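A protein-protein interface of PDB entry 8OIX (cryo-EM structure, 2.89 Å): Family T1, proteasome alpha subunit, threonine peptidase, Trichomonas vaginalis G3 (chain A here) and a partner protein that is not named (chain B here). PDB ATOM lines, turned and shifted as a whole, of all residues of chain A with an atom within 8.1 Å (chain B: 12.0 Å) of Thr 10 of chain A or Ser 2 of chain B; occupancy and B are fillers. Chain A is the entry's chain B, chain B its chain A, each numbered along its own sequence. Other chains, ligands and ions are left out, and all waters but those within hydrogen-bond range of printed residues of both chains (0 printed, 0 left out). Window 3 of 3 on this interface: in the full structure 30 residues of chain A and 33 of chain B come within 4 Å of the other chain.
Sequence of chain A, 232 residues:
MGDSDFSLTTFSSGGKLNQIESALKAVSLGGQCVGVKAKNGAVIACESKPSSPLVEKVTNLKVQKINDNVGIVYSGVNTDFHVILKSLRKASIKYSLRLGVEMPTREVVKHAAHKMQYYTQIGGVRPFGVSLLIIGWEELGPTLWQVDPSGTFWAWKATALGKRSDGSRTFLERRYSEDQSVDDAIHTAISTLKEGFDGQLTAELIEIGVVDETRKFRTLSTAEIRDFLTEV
The side-chain amide nitrogen (NE2) of Gln 19 of chain A is in hydrogen-bond range of the backbone carbonyl oxygen (O) of Phe 12 of chain B.
Among the printed residues, merely in contact across the chains: Pro 127 of chain A with Phe 12 of chain B (3.1 Å), Gln 19 of chain A with Val 11 of chain B (3.5 Å), Leu 8 of chain A with Val 125 of chain B (3.6 Å), Leu 8 of chain A with Leu 9 of chain B (3.7 Å), Leu 8 of chain A with Ser 2 of chain B (3.7 Å), Pro 127 of chain A with Gln 123 of chain B (3.8 Å), Leu 8 of chain A with Val 11 of chain B (3.8 Å) and Thr 10 of chain A with Ser 2 of chain B (3.9 Å).
Printed residues of chain B that touch a printed residue of chain A: Ser 2, Leu 9, Val 11, Phe 12, Gln 123 and Val 125. Hydrophobic or aromatic side chains of chain B within 4 Å of the printed part of chain A: Leu 9, Val 11, Phe 12 and Val 125. Hydrophobic or aromatic side chains of chain A within 4 Å of the printed part of chain B: Leu 8. Among the printed residues, 9 pairs touch across the chains. Among the printed residues, no Asp or Glu carboxylate lies within 4 Å of a Lys or Arg side-chain nitrogen of the other chain.
No residue of chain B comes within 4 Å of Ser 7 of chain A. Of chain B, only Ser 2, Leu 9, Val 11 and Val 125 come within 4 Å of Leu 8 of chain A. No residue of chain B comes within 4 Å of Thr 9 of chain A. Thr 10 of chain A touches one residue of chain B. No residue of chain B comes within 4 Å of Ser 12 of chain A. No residue of chain B comes within 4 Å of Gly 15 of chain A. Leu 17 of chain A touches none of the printed residues of chain B. No residue of chain B comes within 4 Å of Asn 18 of chain A. Gln 19 of chain A touches just these residues of chain B: Val 11 (3.5 Å) and Phe 12 (2.7 Å). Of the printed residues of chain B, Pro 127 of chain A touches Phe 12 and Gln 123. Ser 2 of chain B touches two residues of chain A. Asp 6 of chain B touches none of the printed residues of chain A. Thr 10 of chain B touches none of the printed residues of chain A. Of the printed residues of chain A, Val 11 of chain B touches Leu 8 (3.8 Å) and Gln 19 (3.5 Å). Printed residues of chain A within 4 Å of Phe 12 of chain B: Gln 19 and Pro 127. Printed residues of chain A within 4 Å of Gln 123 of chain B: Pro 127 (3.8 Å). The nearest residue of chain A that does not touch Ser 2 of chain B is Ser 7 of chain A (4.6 Å). The nearest printed residue of chain A that does not touch Phe 12 of chain B is Asn 18 of chain A (5.7 Å).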
ATOM      1  N   PHE A   6      -9.549 -15.934  26.766  1.00  0.00           N
ATOM      2  CA  PHE A   6      -8.791 -15.488  25.610  1.00  0.00           C
ATOM      3  C   PHE A   6      -7.310 -15.387  25.949  1.00  0.00           C
ATOM      4  O   PHE A   6      -6.927 -15.107  27.088  1.00  0.00           O
ATOM      5  CB  PHE A   6      -9.308 -14.139  25.111  1.00  0.00           C
ATOM      6  CG  PHE A   6      -9.308 -13.057  26.152  1.00  0.00           C
ATOM      7  CD1 PHE A   6      -8.169 -12.313  26.406  1.00  0.00           C
ATOM      8  CD2 PHE A   6     -10.455 -12.779  26.874  1.00  0.00           C
ATOM      9  CE1 PHE A   6      -8.172 -11.319  27.361  1.00  0.00           C
ATOM     10  CE2 PHE A   6     -10.465 -11.786  27.830  1.00  0.00           C
ATOM     11  CZ  PHE A   6      -9.323 -11.055  28.074  1.00  0.00           C
ATOM     12  N   SER A   7      -6.476 -15.584  24.934  1.00  0.00           N
ATOM     13  CA  SER A   7      -5.032 -15.575  25.117  1.00  0.00           C
ATOM     14  C   SER A   7      -4.531 -14.139  25.181  1.00  0.00           C
ATOM     15  O   SER A   7      -4.763 -13.352  24.257  1.00  0.00           O
ATOM     16  CB  SER A   7      -4.350 -16.337  23.985  1.00  0.00           C
ATOM     17  OG  SER A   7      -2.948 -16.385  24.174  1.00  0.00           O
ATOM     18  N   LEU A   8      -3.864 -13.790  26.280  1.00  0.00           N
ATOM     19  CA  LEU A   8      -3.235 -12.482  26.397  1.00  0.00           C
ATOM     20  C   LEU A   8      -1.863 -12.437  25.745  1.00  0.00           C
ATOM     21  O   LEU A   8      -1.339 -11.344  25.506  1.00  0.00           O
ATOM     22  CB  LEU A   8      -3.125 -12.082  27.867  1.00  0.00           C
ATOM     23  CG  LEU A   8      -4.464 -11.995  28.594  1.00  0.00           C
ATOM     24  CD1 LEU A   8      -4.680 -13.232  29.442  1.00  0.00           C
ATOM     25  CD2 LEU A   8      -4.532 -10.738  29.439  1.00  0.00           C
ATOM     26  N   THR A   9      -1.273 -13.593  25.456  1.00  0.00           N
ATOM     27  CA  THR A   9      -0.073 -13.672  24.633  1.00  0.00           C
ATOM     28  C   THR A   9      -0.507 -13.940  23.199  1.00  0.00           C
ATOM     29  O   THR A   9      -0.952 -15.045  22.875  1.00  0.00           O
ATOM     30  CB  THR A   9       0.860 -14.768  25.136  1.00  0.00           C
ATOM     31  OG1 THR A   9       1.165 -14.542  26.517  1.00  0.00           O
ATOM     32  CG2 THR A   9       2.150 -14.776  24.331  1.00  0.00           C
ATOM     33  N   THR A  10      -0.395 -12.927  22.346  1.00  0.00           N
ATOM     34  CA  THR A  10      -0.832 -13.034  20.964  1.00  0.00           C
ATOM     35  C   THR A  10       0.216 -12.422  20.051  1.00  0.00           C
ATOM     36  O   THR A  10       0.979 -11.542  20.454  1.00  0.00           O
ATOM     37  CB  THR A  10      -2.180 -12.342  20.734  1.00  0.00           C
ATOM     38  OG1 THR A  10      -2.103 -10.980  21.172  1.00  0.00           O
ATOM     39  CG2 THR A  10      -3.277 -13.055  21.495  1.00  0.00           C
ATOM     40  N   PHE A  11       0.245 -12.908  18.814  1.00  0.00           N
ATOM     41  CA  PHE A  11       1.169 -12.375  17.825  1.00  0.00           C
ATOM     42  C   PHE A  11       0.831 -10.922  17.513  1.00  0.00           C
ATOM     43  O   PHE A  11      -0.335 -10.561  17.341  1.00  0.00           O
ATOM     44  CB  PHE A  11       1.110 -13.208  16.549  1.00  0.00           C
ATOM     45  CG  PHE A  11       1.489 -14.645  16.734  1.00  0.00           C
ATOM     46  CD1 PHE A  11       0.530 -15.592  17.045  1.00  0.00           C
ATOM     47  CD2 PHE A  11       2.800 -15.056  16.570  1.00  0.00           C
ATOM     48  CE1 PHE A  11       0.875 -16.917  17.205  1.00  0.00           C
ATOM     49  CE2 PHE A  11       3.148 -16.379  16.731  1.00  0.00           C
ATOM     50  CZ  PHE A  11       2.185 -17.310  17.049  1.00  0.00           C
ATOM     51  N   SER A  12       1.862 -10.085  17.442  1.00  0.00           N
ATOM     52  CA  SER A  12       1.688  -8.694  17.058  1.00  0.00           C
ATOM     53  C   SER A  12       1.711  -8.577  15.537  1.00  0.00           C
ATOM     54  O   SER A  12       1.889  -9.563  14.817  1.00  0.00           O
ATOM     55  CB  SER A  12       2.762  -7.817  17.700  1.00  0.00           C
ATOM     56  OG  SER A  12       4.051  -8.154  17.220  1.00  0.00           O
ATOM     57  N   SER A  13       1.527  -7.348  15.041  1.00  0.00           N
ATOM     58  CA  SER A  13       1.490  -7.095  13.602  1.00  0.00           C
ATOM     59  C   SER A  13       2.649  -7.745  12.857  1.00  0.00           C
ATOM     60  O   SER A  13       2.495  -8.139  11.696  1.00  0.00           O
ATOM     61  CB  SER A  13       1.482  -5.589  13.335  1.00  0.00           C
ATOM     62  OG  SER A  13       1.434  -5.320  11.945  1.00  0.00           O
ATOM     63  N   GLY A  15       4.476 -10.528  13.886  1.00  0.00           N
ATOM     64  CA  GLY A  15       4.785 -11.875  14.318  1.00  0.00           C
ATOM     65  C   GLY A  15       5.584 -11.945  15.596  1.00  0.00           C
ATOM     66  O   GLY A  15       6.248 -12.954  15.846  1.00  0.00           O
ATOM     67  N   LYS A  16       5.538 -10.899  16.413  1.00  0.00           N
ATOM     68  CA  LYS A  16       6.283 -10.826  17.663  1.00  0.00           C
ATOM     69  C   LYS A  16       5.298 -10.954  18.818  1.00  0.00           C
ATOM     70  O   LYS A  16       4.434 -10.090  19.001  1.00  0.00           O
ATOM     71  CB  LYS A  16       7.067  -9.518  17.750  1.00  0.00           C
ATOM     72  CG  LYS A  16       8.161  -9.517  18.803  1.00  0.00           C
ATOM     73  CD  LYS A  16       9.226 -10.566  18.509  1.00  0.00           C
ATOM     74  CE  LYS A  16       9.768 -10.436  17.094  1.00  0.00           C
ATOM     75  NZ  LYS A  16      10.291  -9.070  16.823  1.00  0.00           N
ATOM     76  N   LEU A  17       5.422 -12.026  19.589  1.00  0.00           N
ATOM     77  CA  LEU A  17       4.582 -12.218  20.768  1.00  0.00           C
ATOM     78  C   LEU A  17       4.989 -11.188  21.811  1.00  0.00           C
ATOM     79  O   LEU A  17       5.976 -11.367  22.527  1.00  0.00           O
ATOM     80  CB  LEU A  17       4.724 -13.633  21.314  1.00  0.00           C
ATOM     81  CG  LEU A  17       4.309 -14.860  20.499  1.00  0.00           C
ATOM     82  CD1 LEU A  17       2.873 -14.724  20.046  1.00  0.00           C
ATOM     83  CD2 LEU A  17       5.240 -15.133  19.325  1.00  0.00           C
ATOM     84  N   ASN A  18       4.229 -10.093  21.891  1.00  0.00           N
ATOM     85  CA  ASN A  18       4.578  -9.007  22.801  1.00  0.00           C
ATOM     86  C   ASN A  18       4.636  -9.466  24.251  1.00  0.00           C
ATOM     87  O   ASN A  18       5.478  -8.985  25.017  1.00  0.00           O
ATOM     88  CB  ASN A  18       3.582  -7.859  22.650  1.00  0.00           C
ATOM     89  CG  ASN A  18       3.856  -7.012  21.428  1.00  0.00           C
ATOM     90  OD1 ASN A  18       4.568  -7.432  20.516  1.00  0.00           O
ATOM     91  ND2 ASN A  18       3.292  -5.811  21.401  1.00  0.00           N
ATOM     92  N   GLN A  19       3.760 -10.389  24.651  1.00  0.00           N
ATOM     93  CA  GLN A  19       3.812 -10.884  26.022  1.00  0.00           C
ATOM     94  C   GLN A  19       5.048 -11.738  26.263  1.00  0.00           C
ATOM     95  O   GLN A  19       5.601 -11.722  27.366  1.00  0.00           O
ATOM     96  CB  GLN A  19       2.546 -11.668  26.354  1.00  0.00           C
ATOM     97  CG  GLN A  19       1.542 -10.886  27.183  1.00  0.00           C
ATOM     98  CD  GLN A  19       2.098 -10.467  28.528  1.00  0.00           C
ATOM     99  OE1 GLN A  19       2.274 -11.291  29.424  1.00  0.00           O
ATOM    100  NE2 GLN A  19       2.378  -9.178  28.677  1.00  0.00           N
ATOM    101  N   ILE A  20       5.498 -12.483  25.252  1.00  0.00           N
ATOM    102  CA  ILE A  20       6.744 -13.231  25.388  1.00  0.00           C
ATOM    103  C   ILE A  20       7.921 -12.284  25.563  1.00  0.00           C
ATOM    104  O   ILE A  20       8.793 -12.507  26.409  1.00  0.00           O
ATOM    105  CB  ILE A  20       6.947 -14.167  24.185  1.00  0.00           C
ATOM    106  CG1 ILE A  20       5.827 -15.198  24.144  1.00  0.00           C
ATOM    107  CG2 ILE A  20       8.302 -14.844  24.261  1.00  0.00           C
ATOM    108  CD1 ILE A  20       5.779 -16.033  25.365  1.00  0.00           C
ATOM    109  N   THR A 120       1.865 -19.717  27.826  1.00  0.00           N
ATOM    110  CA  THR A 120       1.902 -18.708  26.774  1.00  0.00           C
ATOM    111  C   THR A 120       0.771 -18.860  25.770  1.00  0.00           C
ATOM    112  O   THR A 120       0.573 -17.961  24.946  1.00  0.00           O
ATOM    113  CB  THR A 120       3.229 -18.731  26.014  1.00  0.00           C
ATOM    114  OG1 THR A 120       3.294 -19.896  25.184  1.00  0.00           O
ATOM    115  CG2 THR A 120       4.390 -18.708  26.966  1.00  0.00           C
ATOM    116  N   GLN A 121       0.030 -19.964  25.807  1.00  0.00           N
ATOM    117  CA  GLN A 121      -1.044 -20.173  24.848  1.00  0.00           C
ATOM    118  C   GLN A 121      -2.427 -20.135  25.478  1.00  0.00           C
ATOM    119  O   GLN A 121      -3.331 -19.503  24.925  1.00  0.00           O
ATOM    120  CB  GLN A 121      -0.839 -21.502  24.112  1.00  0.00           C
ATOM    121  CG  GLN A 121      -1.637 -21.610  22.829  1.00  0.00           C
ATOM    122  CD  GLN A 121      -0.942 -22.459  21.793  1.00  0.00           C
ATOM    123  OE1 GLN A 121      -0.047 -23.238  22.116  1.00  0.00           O
ATOM    124  NE2 GLN A 121      -1.343 -22.310  20.538  1.00  0.00           N
ATOM    125  N   PRO A 127       2.646 -15.420  30.449  1.00  0.00           N
ATOM    126  CA  PRO A 127       3.781 -16.347  30.449  1.00  0.00           C
ATOM    127  C   PRO A 127       4.585 -16.208  31.730  1.00  0.00           C
ATOM    128  O   PRO A 127       4.637 -15.140  32.343  1.00  0.00           O
ATOM    129  CB  PRO A 127       4.597 -15.920  29.224  1.00  0.00           C
ATOM    130  CG  PRO A 127       3.677 -15.096  28.403  1.00  0.00           C
ATOM    131  CD  PRO A 127       2.744 -14.437  29.359  1.00  0.00           C
ATOM    132  N   SER B   2      -4.398  -6.759  21.948  1.00  0.00           N
ATOM    133  CA  SER B   2      -4.407  -7.097  23.367  1.00  0.00           C
ATOM    134  C   SER B   2      -3.521  -6.144  24.162  1.00  0.00           C
ATOM    135  O   SER B   2      -3.417  -6.250  25.384  1.00  0.00           O
ATOM    136  CB  SER B   2      -3.948  -8.541  23.577  1.00  0.00           C
ATOM    137  OG  SER B   2      -4.027  -8.907  24.942  1.00  0.00           O
ATOM    138  N   SER B   3      -2.883  -5.214  23.455  1.00  0.00           N
ATOM    139  CA  SER B   3      -2.001  -4.251  24.096  1.00  0.00           C
ATOM    140  C   SER B   3      -2.791  -3.309  24.999  1.00  0.00           C
ATOM    141  O   SER B   3      -3.948  -2.976  24.730  1.00  0.00           O
ATOM    142  CB  SER B   3      -1.233  -3.448  23.046  1.00  0.00           C
ATOM    143  OG  SER B   3      -0.387  -2.489  23.656  1.00  0.00           O
ATOM    144  N   GLY B   4      -2.146  -2.880  26.081  1.00  0.00           N
ATOM    145  CA  GLY B   4      -2.756  -2.010  27.061  1.00  0.00           C
ATOM    146  C   GLY B   4      -3.194  -2.699  28.335  1.00  0.00           C
ATOM    147  O   GLY B   4      -3.524  -2.011  29.307  1.00  0.00           O
ATOM    148  N   ALA B   5      -3.202  -4.030  28.361  1.00  0.00           N
ATOM    149  CA  ALA B   5      -3.566  -4.771  29.559  1.00  0.00           C
ATOM    150  C   ALA B   5      -2.431  -4.855  30.568  1.00  0.00           C
ATOM    151  O   ALA B   5      -2.667  -5.272  31.707  1.00  0.00           O
ATOM    152  CB  ALA B   5      -4.022  -6.184  29.189  1.00  0.00           C
ATOM    153  N   ASP B   6      -1.212  -4.476  30.179  1.00  0.00           N
ATOM    154  CA  ASP B   6      -0.061  -4.611  31.061  1.00  0.00           C
ATOM    155  C   ASP B   6      -0.155  -3.725  32.294  1.00  0.00           C
ATOM    156  O   ASP B   6       0.519  -4.002  33.292  1.00  0.00           O
ATOM    157  CB  ASP B   6       1.219  -4.293  30.291  1.00  0.00           C
ATOM    158  CG  ASP B   6       1.204  -2.908  29.681  1.00  0.00           C
ATOM    159  OD1 ASP B   6       0.261  -2.603  28.922  1.00  0.00           O
ATOM    160  OD2 ASP B   6       2.131  -2.120  29.962  1.00  0.00           O
ATOM    161  N   ARG B   7      -0.971  -2.673  32.253  1.00  0.00           N
ATOM    162  CA  ARG B   7      -1.144  -1.792  33.396  1.00  0.00           C
ATOM    163  C   ARG B   7      -2.428  -2.057  34.166  1.00  0.00           C
ATOM    164  O   ARG B   7      -2.501  -1.720  35.353  1.00  0.00           O
ATOM    165  CB  ARG B   7      -1.111  -0.328  32.943  1.00  0.00           C
ATOM    166  CG  ARG B   7      -1.921  -0.052  31.691  1.00  0.00           C
ATOM    167  CD  ARG B   7      -1.768   1.389  31.239  1.00  0.00           C
ATOM    168  NE  ARG B   7      -2.662   1.706  30.132  1.00  0.00           N
ATOM    169  CZ  ARG B   7      -2.363   1.527  28.853  1.00  0.00           C
ATOM    170  NH1 ARG B   7      -1.191   1.042  28.477  1.00  0.00           N
ATOM    171  NH2 ARG B   7      -3.264   1.842  27.926  1.00  0.00           N
ATOM    172  N   TYR B   8      -3.429  -2.660  33.528  1.00  0.00           N
ATOM    173  CA  TYR B   8      -4.708  -2.936  34.169  1.00  0.00           C
ATOM    174  C   TYR B   8      -4.864  -4.390  34.582  1.00  0.00           C
ATOM    175  O   TYR B   8      -5.614  -4.679  35.520  1.00  0.00           O
ATOM    176  CB  TYR B   8      -5.855  -2.547  33.232  1.00  0.00           C
ATOM    177  CG  TYR B   8      -5.726  -1.140  32.703  1.00  0.00           C
ATOM    178  CD1 TYR B   8      -5.744  -0.055  33.561  1.00  0.00           C
ATOM    179  CD2 TYR B   8      -5.573  -0.898  31.348  1.00  0.00           C
ATOM    180  CE1 TYR B   8      -5.618   1.233  33.086  1.00  0.00           C
ATOM    181  CE2 TYR B   8      -5.453   0.386  30.861  1.00  0.00           C
ATOM    182  CZ  TYR B   8      -5.475   1.448  31.735  1.00  0.00           C
ATOM    183  OH  TYR B   8      -5.353   2.732  31.258  1.00  0.00           O
ATOM    184  N   LEU B   9      -4.177  -5.305  33.910  1.00  0.00           N
ATOM    185  CA  LEU B   9      -4.166  -6.713  34.266  1.00  0.00           C
ATOM    186  C   LEU B   9      -2.759  -7.106  34.688  1.00  0.00           C
ATOM    187  O   LEU B   9      -1.784  -6.394  34.435  1.00  0.00           O
ATOM    188  CB  LEU B   9      -4.641  -7.591  33.102  1.00  0.00           C
ATOM    189  CG  LEU B   9      -6.074  -7.377  32.619  1.00  0.00           C
ATOM    190  CD1 LEU B   9      -6.394  -8.321  31.479  1.00  0.00           C
ATOM    191  CD2 LEU B   9      -7.042  -7.580  33.764  1.00  0.00           C
ATOM    192  N   THR B  10      -2.658  -8.261  35.343  1.00  0.00           N
ATOM    193  CA  THR B  10      -1.374  -8.749  35.839  1.00  0.00           C
ATOM    194  C   THR B  10      -0.641  -9.522  34.739  1.00  0.00           C
ATOM    195  O   THR B  10      -0.415 -10.732  34.806  1.00  0.00           O
ATOM    196  CB  THR B  10      -1.573  -9.579  37.100  1.00  0.00           C
ATOM    197  OG1 THR B  10      -0.319 -10.138  37.504  1.00  0.00           O
ATOM    198  CG2 THR B  10      -2.610 -10.680  36.889  1.00  0.00           C
ATOM    199  N   VAL B  11      -0.253  -8.781  33.704  1.00  0.00           N
ATOM    200  CA  VAL B  11       0.627  -9.280  32.658  1.00  0.00           C
ATOM    201  C   VAL B  11       1.810  -8.332  32.551  1.00  0.00           C
ATOM    202  O   VAL B  11       1.721  -7.155  32.912  1.00  0.00           O
ATOM    203  CB  VAL B  11      -0.079  -9.426  31.290  1.00  0.00           C
ATOM    204  CG1 VAL B  11      -1.270 -10.337  31.403  1.00  0.00           C
ATOM    205  CG2 VAL B  11      -0.503  -8.077  30.760  1.00  0.00           C
ATOM    206  N   PHE B  12       2.928  -8.859  32.064  1.00  0.00           N
ATOM    207  CA  PHE B  12       4.158  -8.084  32.016  1.00  0.00           C
ATOM    208  C   PHE B  12       4.024  -6.921  31.043  1.00  0.00           C
ATOM    209  O   PHE B  12       3.384  -7.033  29.995  1.00  0.00           O
ATOM    210  CB  PHE B  12       5.327  -8.978  31.612  1.00  0.00           C
ATOM    211  CG  PHE B  12       5.633 -10.048  32.607  1.00  0.00           C
ATOM    212  CD1 PHE B  12       6.152  -9.727  33.846  1.00  0.00           C
ATOM    213  CD2 PHE B  12       5.388 -11.375  32.311  1.00  0.00           C
ATOM    214  CE1 PHE B  12       6.431 -10.708  34.767  1.00  0.00           C
ATOM    215  CE2 PHE B  12       5.663 -12.359  33.230  1.00  0.00           C
ATOM    216  CZ  PHE B  12       6.184 -12.026  34.460  1.00  0.00           C
ATOM    217  N   SER B  13       4.632  -5.797  31.401  1.00  0.00           N
ATOM    218  CA  SER B  13       4.672  -4.630  30.539  1.00  0.00           C
ATOM    219  C   SER B  13       5.840  -4.726  29.565  1.00  0.00           C
ATOM    220  O   SER B  13       6.675  -5.627  29.642  1.00  0.00           O
ATOM    221  CB  SER B  13       4.776  -3.357  31.375  1.00  0.00           C
ATOM    222  OG  SER B  13       5.887  -3.418  32.249  1.00  0.00           O
ATOM    223  N   ALA B  14       5.892  -3.767  28.636  1.00  0.00           N
ATOM    224  CA  ALA B  14       6.986  -3.730  27.672  1.00  0.00           C
ATOM    225  C   ALA B  14       8.339  -3.698  28.369  1.00  0.00           C
ATOM    226  O   ALA B  14       9.330  -4.197  27.826  1.00  0.00           O
ATOM    227  CB  ALA B  14       6.834  -2.524  26.747  1.00  0.00           C
ATOM    228  N   TRP B  19       2.756  -4.413  36.664  1.00  0.00           N
ATOM    229  CA  TRP B  19       2.320  -3.152  37.252  1.00  0.00           C
ATOM    230  C   TRP B  19       1.261  -3.371  38.322  1.00  0.00           C
ATOM    231  O   TRP B  19       1.249  -2.676  39.344  1.00  0.00           O
ATOM    232  CB  TRP B  19       1.801  -2.222  36.159  1.00  0.00           C
ATOM    233  CG  TRP B  19       2.899  -1.590  35.374  1.00  0.00           C
ATOM    234  CD1 TRP B  19       3.160  -1.760  34.049  1.00  0.00           C
ATOM    235  CD2 TRP B  19       3.904  -0.699  35.871  1.00  0.00           C
ATOM    236  NE1 TRP B  19       4.259  -1.022  33.684  1.00  0.00           N
ATOM    237  CE2 TRP B  19       4.734  -0.361  34.786  1.00  0.00           C
ATOM    238  CE3 TRP B  19       4.178  -0.149  37.126  1.00  0.00           C
ATOM    239  CZ2 TRP B  19       5.819   0.501  34.918  1.00  0.00           C
ATOM    240  CZ3 TRP B  19       5.255   0.705  37.254  1.00  0.00           C
ATOM    241  CH2 TRP B  19       6.062   1.022  36.157  1.00  0.00           C
ATOM    242  N   GLN B 123      -0.395 -14.206  38.035  1.00  0.00           N
ATOM    243  CA  GLN B 123      -0.408 -14.827  36.718  1.00  0.00           C
ATOM    244  C   GLN B 123      -1.798 -14.906  36.110  1.00  0.00           C
ATOM    245  O   GLN B 123      -1.995 -14.488  34.966  1.00  0.00           O
ATOM    246  CB  GLN B 123       0.207 -16.229  36.793  1.00  0.00           C
ATOM    247  CG  GLN B 123       0.448 -16.862  35.442  1.00  0.00           C
ATOM    248  CD  GLN B 123       1.646 -17.778  35.451  1.00  0.00           C
ATOM    249  OE1 GLN B 123       1.926 -18.435  36.451  1.00  0.00           O
ATOM    250  NE2 GLN B 123       2.372 -17.815  34.342  1.00  0.00           N
ATOM    251  N   VAL B 125      -4.884 -13.524  35.044  1.00  0.00           N
ATOM    252  CA  VAL B 125      -5.248 -12.130  34.829  1.00  0.00           C
ATOM    253  C   VAL B 125      -6.636 -11.797  35.344  1.00  0.00           C
ATOM    254  O   VAL B 125      -6.969 -10.616  35.479  1.00  0.00           O
ATOM    255  CB  VAL B 125      -5.154 -11.781  33.333  1.00  0.00           C
ATOM    256  CG1 VAL B 125      -3.814 -12.211  32.795  1.00  0.00           C
ATOM    257  CG2 VAL B 125      -6.278 -12.437  32.567  1.00  0.00           C
ATOM    258  N   TYR B 126      -7.452 -12.806  35.629  1.00  0.00           N
ATOM    259  CA  TYR B 126      -8.783 -12.604  36.176  1.00  0.00           C
ATOM    260  C   TYR B 126      -8.790 -12.613  37.698  1.00  0.00           C
ATOM    261  O   TYR B 126      -9.867 -12.585  38.301  1.00  0.00           O
ATOM    262  CB  TYR B 126      -9.740 -13.669  35.633  1.00  0.00           C
ATOM    263  CG  TYR B 126      -9.345 -15.090  35.966  1.00  0.00           C
ATOM    264  CD1 TYR B 126      -9.806 -15.708  37.121  1.00  0.00           C
ATOM    265  CD2 TYR B 126      -8.506 -15.813  35.128  1.00  0.00           C
ATOM    266  CE1 TYR B 126      -9.448 -17.004  37.429  1.00  0.00           C
ATOM    267  CE2 TYR B 126      -8.142 -17.109  35.429  1.00  0.00           C
ATOM    268  CZ  TYR B 126      -8.615 -17.699  36.581  1.00  0.00           C
ATOM    269  OH  TYR B 126      -8.256 -18.992  36.886  1.00  0.00           O
